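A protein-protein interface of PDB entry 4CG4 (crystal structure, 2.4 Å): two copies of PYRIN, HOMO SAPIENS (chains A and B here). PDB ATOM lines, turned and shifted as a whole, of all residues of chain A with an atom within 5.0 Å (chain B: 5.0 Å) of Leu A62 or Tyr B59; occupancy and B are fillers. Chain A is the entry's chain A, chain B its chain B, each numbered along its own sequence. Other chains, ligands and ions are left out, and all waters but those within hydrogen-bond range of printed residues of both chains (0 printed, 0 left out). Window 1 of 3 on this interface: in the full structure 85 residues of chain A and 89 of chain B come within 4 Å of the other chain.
Printed residues of chain B that touch a printed residue of chain A: Leu B55, Val B58, Tyr B59, Leu B62 and Phe B163. Hydrophobic or aromatic side chains of chain B that line the printed part of chain A: Leu B55, Val B58, Tyr B59, Leu B62 and Phe B163. Along chain B the printed residues that touch a printed residue of chain A span positions 55 to 163. Printed residues of chain A that touch a printed residue of chain B: Tyr A59, Leu A62, Glu A63 and Glu A66. Among the printed residues, 7 pairs touch across the chains.
Of chain B, only Val B58 (3.8 Å), Tyr B59 (3.4 Å), Leu B62 (3.6 Å) and Phe B163 (3.7 Å) come within 4 Å of Leu A62. Printed residues of chain B within 4 Å of Glu A66: Leu B55. Of the printed residues of chain A, Phe B163 touches Leu A62 (3.7 Å). Of the printed residues of chain B, Tyr A59 touches Leu B62. Thr A160 touches none of the printed residues of chain B. The nearest residue of chain B that does not touch Leu A62 is Leu B55 (4.8 Å). The nearest printed residue of chain B that does not touch Glu A63 is Leu B55 (7.4 Å).
Tyr A59 touches Leu B62, and with the chains exchanged Leu A62 touches Tyr B59. Leu A62 touches Val B58, but with the chains exchanged Val A58 does not touch Leu B62 (4.2 Å). Leu B62 touches its own counterpart, Leu A62. Glu A63 touches Tyr B59, but with the chains exchanged Tyr A59 does not touch Glu B63 (5.2 Å). Positions printed for both chains: 58, 59, 60, 61, 62, 63 and 64.
Tyr A59 touches Leu B62. Val B58 touches Leu A62. Leu A62 touches Tyr B59 (CB to OH, 3.4 Å). Leu A62 touches Leu B62. Leu A62 touches Phe B163. Tyr B59 touches Glu A63 (OH to N, 3.97 Å). Leu B55 touches Glu A66.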
ATOM      1  N   VAL A  58      20.084  -0.111   0.868  1.00  0.00           N
ATOM      2  CA  VAL A  58      19.313   0.886   1.601  1.00  0.00           C
ATOM      3  C   VAL A  58      19.611   0.898   3.094  1.00  0.00           C
ATOM      4  O   VAL A  58      19.765   1.970   3.673  1.00  0.00           O
ATOM      5  CB  VAL A  58      17.809   0.701   1.366  1.00  0.00           C
ATOM      6  CG1 VAL A  58      16.961   1.487   2.372  1.00  0.00           C
ATOM      7  CG2 VAL A  58      17.498   1.112  -0.052  1.00  0.00           C
ATOM      8  N   TYR A  59      19.632  -0.270   3.723  1.00  0.00           N
ATOM      9  CA  TYR A  59      19.883  -0.345   5.149  1.00  0.00           C
ATOM     10  C   TYR A  59      21.231   0.302   5.439  1.00  0.00           C
ATOM     11  O   TYR A  59      21.365   1.063   6.405  1.00  0.00           O
ATOM     12  CB  TYR A  59      19.889  -1.782   5.637  1.00  0.00           C
ATOM     13  CG  TYR A  59      18.546  -2.456   5.535  1.00  0.00           C
ATOM     14  CD1 TYR A  59      17.364  -1.766   5.778  1.00  0.00           C
ATOM     15  CD2 TYR A  59      18.467  -3.792   5.181  1.00  0.00           C
ATOM     16  CE1 TYR A  59      16.141  -2.397   5.669  1.00  0.00           C
ATOM     17  CE2 TYR A  59      17.261  -4.432   5.072  1.00  0.00           C
ATOM     18  CZ  TYR A  59      16.096  -3.739   5.315  1.00  0.00           C
ATOM     19  OH  TYR A  59      14.895  -4.410   5.192  1.00  0.00           O
ATOM     20  N   TYR A  60      22.212  -0.007   4.588  1.00  0.00           N
ATOM     21  CA  TYR A  60      23.536   0.551   4.718  1.00  0.00           C
ATOM     22  C   TYR A  60      23.480   2.065   4.668  1.00  0.00           C
ATOM     23  O   TYR A  60      23.978   2.730   5.580  1.00  0.00           O
ATOM     24  CB  TYR A  60      24.469   0.009   3.636  1.00  0.00           C
ATOM     25  CG  TYR A  60      25.843   0.654   3.664  1.00  0.00           C
ATOM     26  CD1 TYR A  60      26.743   0.346   4.679  1.00  0.00           C
ATOM     27  CD2 TYR A  60      26.254   1.539   2.662  1.00  0.00           C
ATOM     28  CE1 TYR A  60      28.011   0.929   4.727  1.00  0.00           C
ATOM     29  CE2 TYR A  60      27.542   2.112   2.688  1.00  0.00           C
ATOM     30  CZ  TYR A  60      28.408   1.797   3.728  1.00  0.00           C
ATOM     31  OH  TYR A  60      29.674   2.348   3.792  1.00  0.00           O
ATOM     32  N   PHE A  61      22.844   2.596   3.627  1.00  0.00           N
ATOM     33  CA  PHE A  61      22.667   4.031   3.515  1.00  0.00           C
ATOM     34  C   PHE A  61      22.046   4.598   4.795  1.00  0.00           C
ATOM     35  O   PHE A  61      22.528   5.634   5.305  1.00  0.00           O
ATOM     36  CB  PHE A  61      21.805   4.419   2.325  1.00  0.00           C
ATOM     37  CG  PHE A  61      22.420   4.112   0.985  1.00  0.00           C
ATOM     38  CD1 PHE A  61      23.793   4.053   0.818  1.00  0.00           C
ATOM     39  CD2 PHE A  61      21.598   3.888  -0.126  1.00  0.00           C
ATOM     40  CE1 PHE A  61      24.348   3.772  -0.429  1.00  0.00           C
ATOM     41  CE2 PHE A  61      22.139   3.615  -1.367  1.00  0.00           C
ATOM     42  CZ  PHE A  61      23.518   3.550  -1.526  1.00  0.00           C
ATOM     43  N   LEU A  62      20.976   3.981   5.300  1.00  0.00           N
ATOM     44  CA  LEU A  62      20.372   4.500   6.537  1.00  0.00           C
ATOM     45  C   LEU A  62      21.328   4.474   7.742  1.00  0.00           C
ATOM     46  O   LEU A  62      21.342   5.426   8.547  1.00  0.00           O
ATOM     47  CB  LEU A  62      19.098   3.748   6.887  1.00  0.00           C
ATOM     48  CG  LEU A  62      17.934   4.079   5.940  1.00  0.00           C
ATOM     49  CD1 LEU A  62      16.688   3.271   6.260  1.00  0.00           C
ATOM     50  CD2 LEU A  62      17.596   5.557   5.964  1.00  0.00           C
ATOM     51  N   GLU A  63      22.105   3.396   7.869  1.00  0.00           N
ATOM     52  CA  GLU A  63      23.073   3.295   8.948  1.00  0.00           C
ATOM     53  C   GLU A  63      24.060   4.481   8.843  1.00  0.00           C
ATOM     54  O   GLU A  63      24.370   5.175   9.833  1.00  0.00           O
ATOM     55  CB  GLU A  63      23.797   1.945   8.869  1.00  0.00           C
ATOM     56  CG  GLU A  63      22.891   0.755   9.230  1.00  0.00           C
ATOM     57  CD  GLU A  63      23.429  -0.602   8.749  1.00  0.00           C
ATOM     58  OE1 GLU A  63      24.593  -0.684   8.304  1.00  0.00           O
ATOM     59  OE2 GLU A  63      22.687  -1.598   8.833  1.00  0.00           O
ATOM     60  N   GLN A  64      24.501   4.736   7.618  1.00  0.00           N
ATOM     61  CA  GLN A  64      25.355   5.864   7.356  1.00  0.00           C
ATOM     62  C   GLN A  64      24.683   7.204   7.741  1.00  0.00           C
ATOM     63  O   GLN A  64      25.302   8.018   8.425  1.00  0.00           O
ATOM     64  CB  GLN A  64      25.797   5.849   5.894  1.00  0.00           C
ATOM     65  CG  GLN A  64      26.697   4.650   5.577  1.00  0.00           C
ATOM     66  CD  GLN A  64      27.992   4.612   6.405  1.00  0.00           C
ATOM     67  OE1 GLN A  64      28.889   5.433   6.227  1.00  0.00           O
ATOM     68  NE2 GLN A  64      28.075   3.650   7.325  1.00  0.00           N
ATOM     69  N   GLN A  65      23.446   7.458   7.327  1.00  0.00           N
ATOM     70  CA  GLN A  65      22.806   8.690   7.791  1.00  0.00           C
ATOM     71  C   GLN A  65      22.743   8.801   9.309  1.00  0.00           C
ATOM     72  O   GLN A  65      23.042   9.872   9.883  1.00  0.00           O
ATOM     73  CB  GLN A  65      21.370   8.856   7.320  1.00  0.00           C
ATOM     74  CG  GLN A  65      21.182   9.337   5.918  1.00  0.00           C
ATOM     75  CD  GLN A  65      19.794   9.973   5.665  1.00  0.00           C
ATOM     76  OE1 GLN A  65      19.520  10.402   4.555  1.00  0.00           O
ATOM     77  NE2 GLN A  65      18.958  10.093   6.698  1.00  0.00           N
ATOM     78  N   GLU A  66      22.349   7.716   9.970  1.00  0.00           N
ATOM     79  CA  GLU A  66      22.254   7.776  11.419  1.00  0.00           C
ATOM     80  C   GLU A  66      23.614   8.143  12.037  1.00  0.00           C
ATOM     81  O   GLU A  66      23.664   8.959  12.950  1.00  0.00           O
ATOM     82  CB  GLU A  66      21.713   6.481  11.973  1.00  0.00           C
ATOM     83  CG  GLU A  66      21.303   6.567  13.430  1.00  0.00           C
ATOM     84  CD  GLU A  66      20.579   5.329  13.892  1.00  0.00           C
ATOM     85  OE1 GLU A  66      19.369   5.197  13.542  1.00  0.00           O
ATOM     86  OE2 GLU A  66      21.197   4.501  14.593  1.00  0.00           O
ATOM     87  N   HIS A  67      24.700   7.541  11.552  1.00  0.00           N
ATOM     88  CA  HIS A  67      26.032   7.881  12.065  1.00  0.00           C
ATOM     89  C   HIS A  67      26.374   9.356  11.807  1.00  0.00           C
ATOM     90  O   HIS A  67      26.849  10.059  12.702  1.00  0.00           O
ATOM     91  CB  HIS A  67      27.110   6.968  11.465  1.00  0.00           C
ATOM     92  CG  HIS A  67      27.006   5.545  11.951  1.00  0.00           C
ATOM     93  ND1 HIS A  67      26.836   5.227  13.264  1.00  0.00           N
ATOM     94  CD2 HIS A  67      27.070   4.373  11.259  1.00  0.00           C
ATOM     95  CE1 HIS A  67      26.776   3.900  13.390  1.00  0.00           C
ATOM     96  NE2 HIS A  67      26.919   3.372  12.200  1.00  0.00           N
ATOM     97  N   THR A 160      14.907  11.179   3.700  1.00  0.00           N
ATOM     98  CA  THR A 160      13.884  10.180   4.028  1.00  0.00           C
ATOM     99  C   THR A 160      12.388  10.453   3.703  1.00  0.00           C
ATOM    100  O   THR A 160      11.637   9.507   3.441  1.00  0.00           O
ATOM    101  CB  THR A 160      13.950   9.833   5.534  1.00  0.00           C
ATOM    102  OG1 THR A 160      13.694  10.996   6.330  1.00  0.00           O
ATOM    103  CG2 THR A 160      15.288   9.249   5.868  1.00  0.00           C
ATOM    104  N   LEU B  55      13.382   8.443  11.736  1.00  0.00           N
ATOM    105  CA  LEU B  55      14.099   7.212  11.485  1.00  0.00           C
ATOM    106  C   LEU B  55      13.280   6.009  11.971  1.00  0.00           C
ATOM    107  O   LEU B  55      13.195   4.994  11.274  1.00  0.00           O
ATOM    108  CB  LEU B  55      15.467   7.208  12.139  1.00  0.00           C
ATOM    109  CG  LEU B  55      16.483   8.148  11.504  1.00  0.00           C
ATOM    110  CD1 LEU B  55      17.823   8.012  12.239  1.00  0.00           C
ATOM    111  CD2 LEU B  55      16.654   7.966  10.014  1.00  0.00           C
ATOM    112  N   GLU B  56      12.708   6.121  13.168  1.00  0.00           N
ATOM    113  CA  GLU B  56      11.892   5.053  13.734  1.00  0.00           C
ATOM    114  C   GLU B  56      10.752   4.641  12.771  1.00  0.00           C
ATOM    115  O   GLU B  56      10.488   3.439  12.522  1.00  0.00           O
ATOM    116  CB  GLU B  56      11.319   5.531  15.075  1.00  0.00           C
ATOM    117  CG  GLU B  56      12.280   5.419  16.274  1.00  0.00           C
ATOM    118  CD  GLU B  56      11.743   6.078  17.557  1.00  0.00           C
ATOM    119  OE1 GLU B  56      10.572   6.513  17.577  1.00  0.00           O
ATOM    120  OE2 GLU B  56      12.499   6.162  18.550  1.00  0.00           O
ATOM    121  N   GLN B  57      10.102   5.652  12.214  1.00  0.00           N
ATOM    122  CA  GLN B  57       9.033   5.432  11.275  1.00  0.00           C
ATOM    123  C   GLN B  57       9.527   4.696   9.988  1.00  0.00           C
ATOM    124  O   GLN B  57       8.937   3.651   9.561  1.00  0.00           O
ATOM    125  CB  GLN B  57       8.364   6.789  10.980  1.00  0.00           C
ATOM    126  CG  GLN B  57       6.952   6.695  10.409  1.00  0.00           C
ATOM    127  CD  GLN B  57       5.930   6.033  11.382  1.00  0.00           C
ATOM    128  OE1 GLN B  57       6.275   5.605  12.489  1.00  0.00           O
ATOM    129  NE2 GLN B  57       4.673   5.957  10.954  1.00  0.00           N
ATOM    130  N   VAL B  58      10.610   5.188   9.389  1.00  0.00           N
ATOM    131  CA  VAL B  58      11.155   4.504   8.222  1.00  0.00           C
ATOM    132  C   VAL B  58      11.496   3.050   8.554  1.00  0.00           C
ATOM    133  O   VAL B  58      11.091   2.119   7.827  1.00  0.00           O
ATOM    134  CB  VAL B  58      12.395   5.209   7.666  1.00  0.00           C
ATOM    135  CG1 VAL B  58      13.025   4.416   6.518  1.00  0.00           C
ATOM    136  CG2 VAL B  58      12.001   6.522   7.135  1.00  0.00           C
ATOM    137  N   TYR B  59      12.229   2.840   9.638  1.00  0.00           N
ATOM    138  CA  TYR B  59      12.600   1.474  10.025  1.00  0.00           C
ATOM    139  C   TYR B  59      11.370   0.591  10.205  1.00  0.00           C
ATOM    140  O   TYR B  59      11.385  -0.566   9.794  1.00  0.00           O
ATOM    141  CB  TYR B  59      13.465   1.482  11.289  1.00  0.00           C
ATOM    142  CG  TYR B  59      14.914   1.830  11.005  1.00  0.00           C
ATOM    143  CD1 TYR B  59      15.739   0.921  10.333  1.00  0.00           C
ATOM    144  CD2 TYR B  59      15.441   3.083  11.334  1.00  0.00           C
ATOM    145  CE1 TYR B  59      17.079   1.229  10.054  1.00  0.00           C
ATOM    146  CE2 TYR B  59      16.762   3.412  11.051  1.00  0.00           C
ATOM    147  CZ  TYR B  59      17.579   2.486  10.411  1.00  0.00           C
ATOM    148  OH  TYR B  59      18.894   2.814  10.137  1.00  0.00           O
ATOM    149  N   TYR B  60      10.317   1.117  10.825  1.00  0.00           N
ATOM    150  CA  TYR B  60       9.093   0.345  10.962  1.00  0.00           C
ATOM    151  C   TYR B  60       8.546  -0.134   9.621  1.00  0.00           C
ATOM    152  O   TYR B  60       8.362  -1.331   9.428  1.00  0.00           O
ATOM    153  CB  TYR B  60       8.011   1.167  11.658  1.00  0.00           C
ATOM    154  CG  TYR B  60       6.653   0.492  11.605  1.00  0.00           C
ATOM    155  CD1 TYR B  60       6.339  -0.588  12.424  1.00  0.00           C
ATOM    156  CD2 TYR B  60       5.692   0.934  10.708  1.00  0.00           C
ATOM    157  CE1 TYR B  60       5.086  -1.192  12.364  1.00  0.00           C
ATOM    158  CE2 TYR B  60       4.440   0.335  10.631  1.00  0.00           C
ATOM    159  CZ  TYR B  60       4.136  -0.726  11.455  1.00  0.00           C
ATOM    160  OH  TYR B  60       2.883  -1.304  11.355  1.00  0.00           O
ATOM    161  N   PHE B  61       8.317   0.796   8.697  1.00  0.00           N
ATOM    162  CA  PHE B  61       7.833   0.412   7.370  1.00  0.00           C
ATOM    163  C   PHE B  61       8.747  -0.621   6.699  1.00  0.00           C
ATOM    164  O   PHE B  61       8.256  -1.605   6.145  1.00  0.00           O
ATOM    165  CB  PHE B  61       7.638   1.654   6.493  1.00  0.00           C
ATOM    166  CG  PHE B  61       6.487   2.539   6.940  1.00  0.00           C
ATOM    167  CD1 PHE B  61       5.342   1.998   7.508  1.00  0.00           C
ATOM    168  CD2 PHE B  61       6.592   3.924   6.880  1.00  0.00           C
ATOM    169  CE1 PHE B  61       4.308   2.822   7.937  1.00  0.00           C
ATOM    170  CE2 PHE B  61       5.560   4.741   7.320  1.00  0.00           C
ATOM    171  CZ  PHE B  61       4.431   4.195   7.853  1.00  0.00           C
ATOM    172  N   LEU B  62      10.056  -0.386   6.700  1.00  0.00           N
ATOM    173  CA  LEU B  62      10.994  -1.351   6.109  1.00  0.00           C
ATOM    174  C   LEU B  62      10.951  -2.737   6.775  1.00  0.00           C
ATOM    175  O   LEU B  62      11.059  -3.761   6.086  1.00  0.00           O
ATOM    176  CB  LEU B  62      12.415  -0.813   6.166  1.00  0.00           C
ATOM    177  CG  LEU B  62      12.802   0.318   5.218  1.00  0.00           C
ATOM    178  CD1 LEU B  62      14.228   0.803   5.546  1.00  0.00           C
ATOM    179  CD2 LEU B  62      12.740  -0.121   3.749  1.00  0.00           C
ATOM    180  N   GLU B  63      10.849  -2.791   8.101  1.00  0.00           N
ATOM    181  CA  GLU B  63      10.739  -4.097   8.749  1.00  0.00           C
ATOM    182  C   GLU B  63       9.466  -4.803   8.295  1.00  0.00           C
ATOM    183  O   GLU B  63       9.479  -6.017   8.043  1.00  0.00           O
ATOM    184  CB  GLU B  63      10.789  -4.008  10.277  1.00  0.00           C
ATOM    185  CG  GLU B  63      12.165  -3.679  10.808  1.00  0.00           C
ATOM    186  CD  GLU B  63      12.162  -3.343  12.284  1.00  0.00           C
ATOM    187  OE1 GLU B  63      11.130  -3.627  12.940  1.00  0.00           O
ATOM    188  OE2 GLU B  63      13.183  -2.787  12.777  1.00  0.00           O
ATOM    189  N   GLN B  64       8.374  -4.052   8.210  1.00  0.00           N
ATOM    190  CA  GLN B  64       7.139  -4.610   7.681  1.00  0.00           C
ATOM    191  C   GLN B  64       7.324  -5.138   6.254  1.00  0.00           C
ATOM    192  O   GLN B  64       6.930  -6.278   5.943  1.00  0.00           O
ATOM    193  CB  GLN B  64       6.024  -3.575   7.692  1.00  0.00           C
ATOM    194  CG  GLN B  64       5.591  -3.163   9.083  1.00  0.00           C
ATOM    195  CD  GLN B  64       5.058  -4.313   9.886  1.00  0.00           C
ATOM    196  OE1 GLN B  64       3.997  -4.853   9.589  1.00  0.00           O
ATOM    197  NE2 GLN B  64       5.790  -4.692  10.928  1.00  0.00           N
ATOM    198  N   PHE B 163      15.035   6.923  -3.526  1.00  0.00           N
ATOM    199  CA  PHE B 163      15.685   7.204  -2.262  1.00  0.00           C
ATOM    200  C   PHE B 163      17.206   7.391  -2.443  1.00  0.00           C
ATOM    201  O   PHE B 163      17.806   8.322  -1.878  1.00  0.00           O
ATOM    202  CB  PHE B 163      15.420   6.087  -1.282  1.00  0.00           C
ATOM    203  CG  PHE B 163      16.203   6.209  -0.005  1.00  0.00           C
ATOM    204  CD1 PHE B 163      15.996   7.276   0.860  1.00  0.00           C
ATOM    205  CD2 PHE B 163      17.149   5.251   0.331  1.00  0.00           C
ATOM    206  CE1 PHE B 163      16.725   7.386   2.037  1.00  0.00           C
ATOM    207  CE2 PHE B 163      17.874   5.355   1.498  1.00  0.00           C
ATOM    208  CZ  PHE B 163      17.662   6.425   2.357  1.00  0.00           C
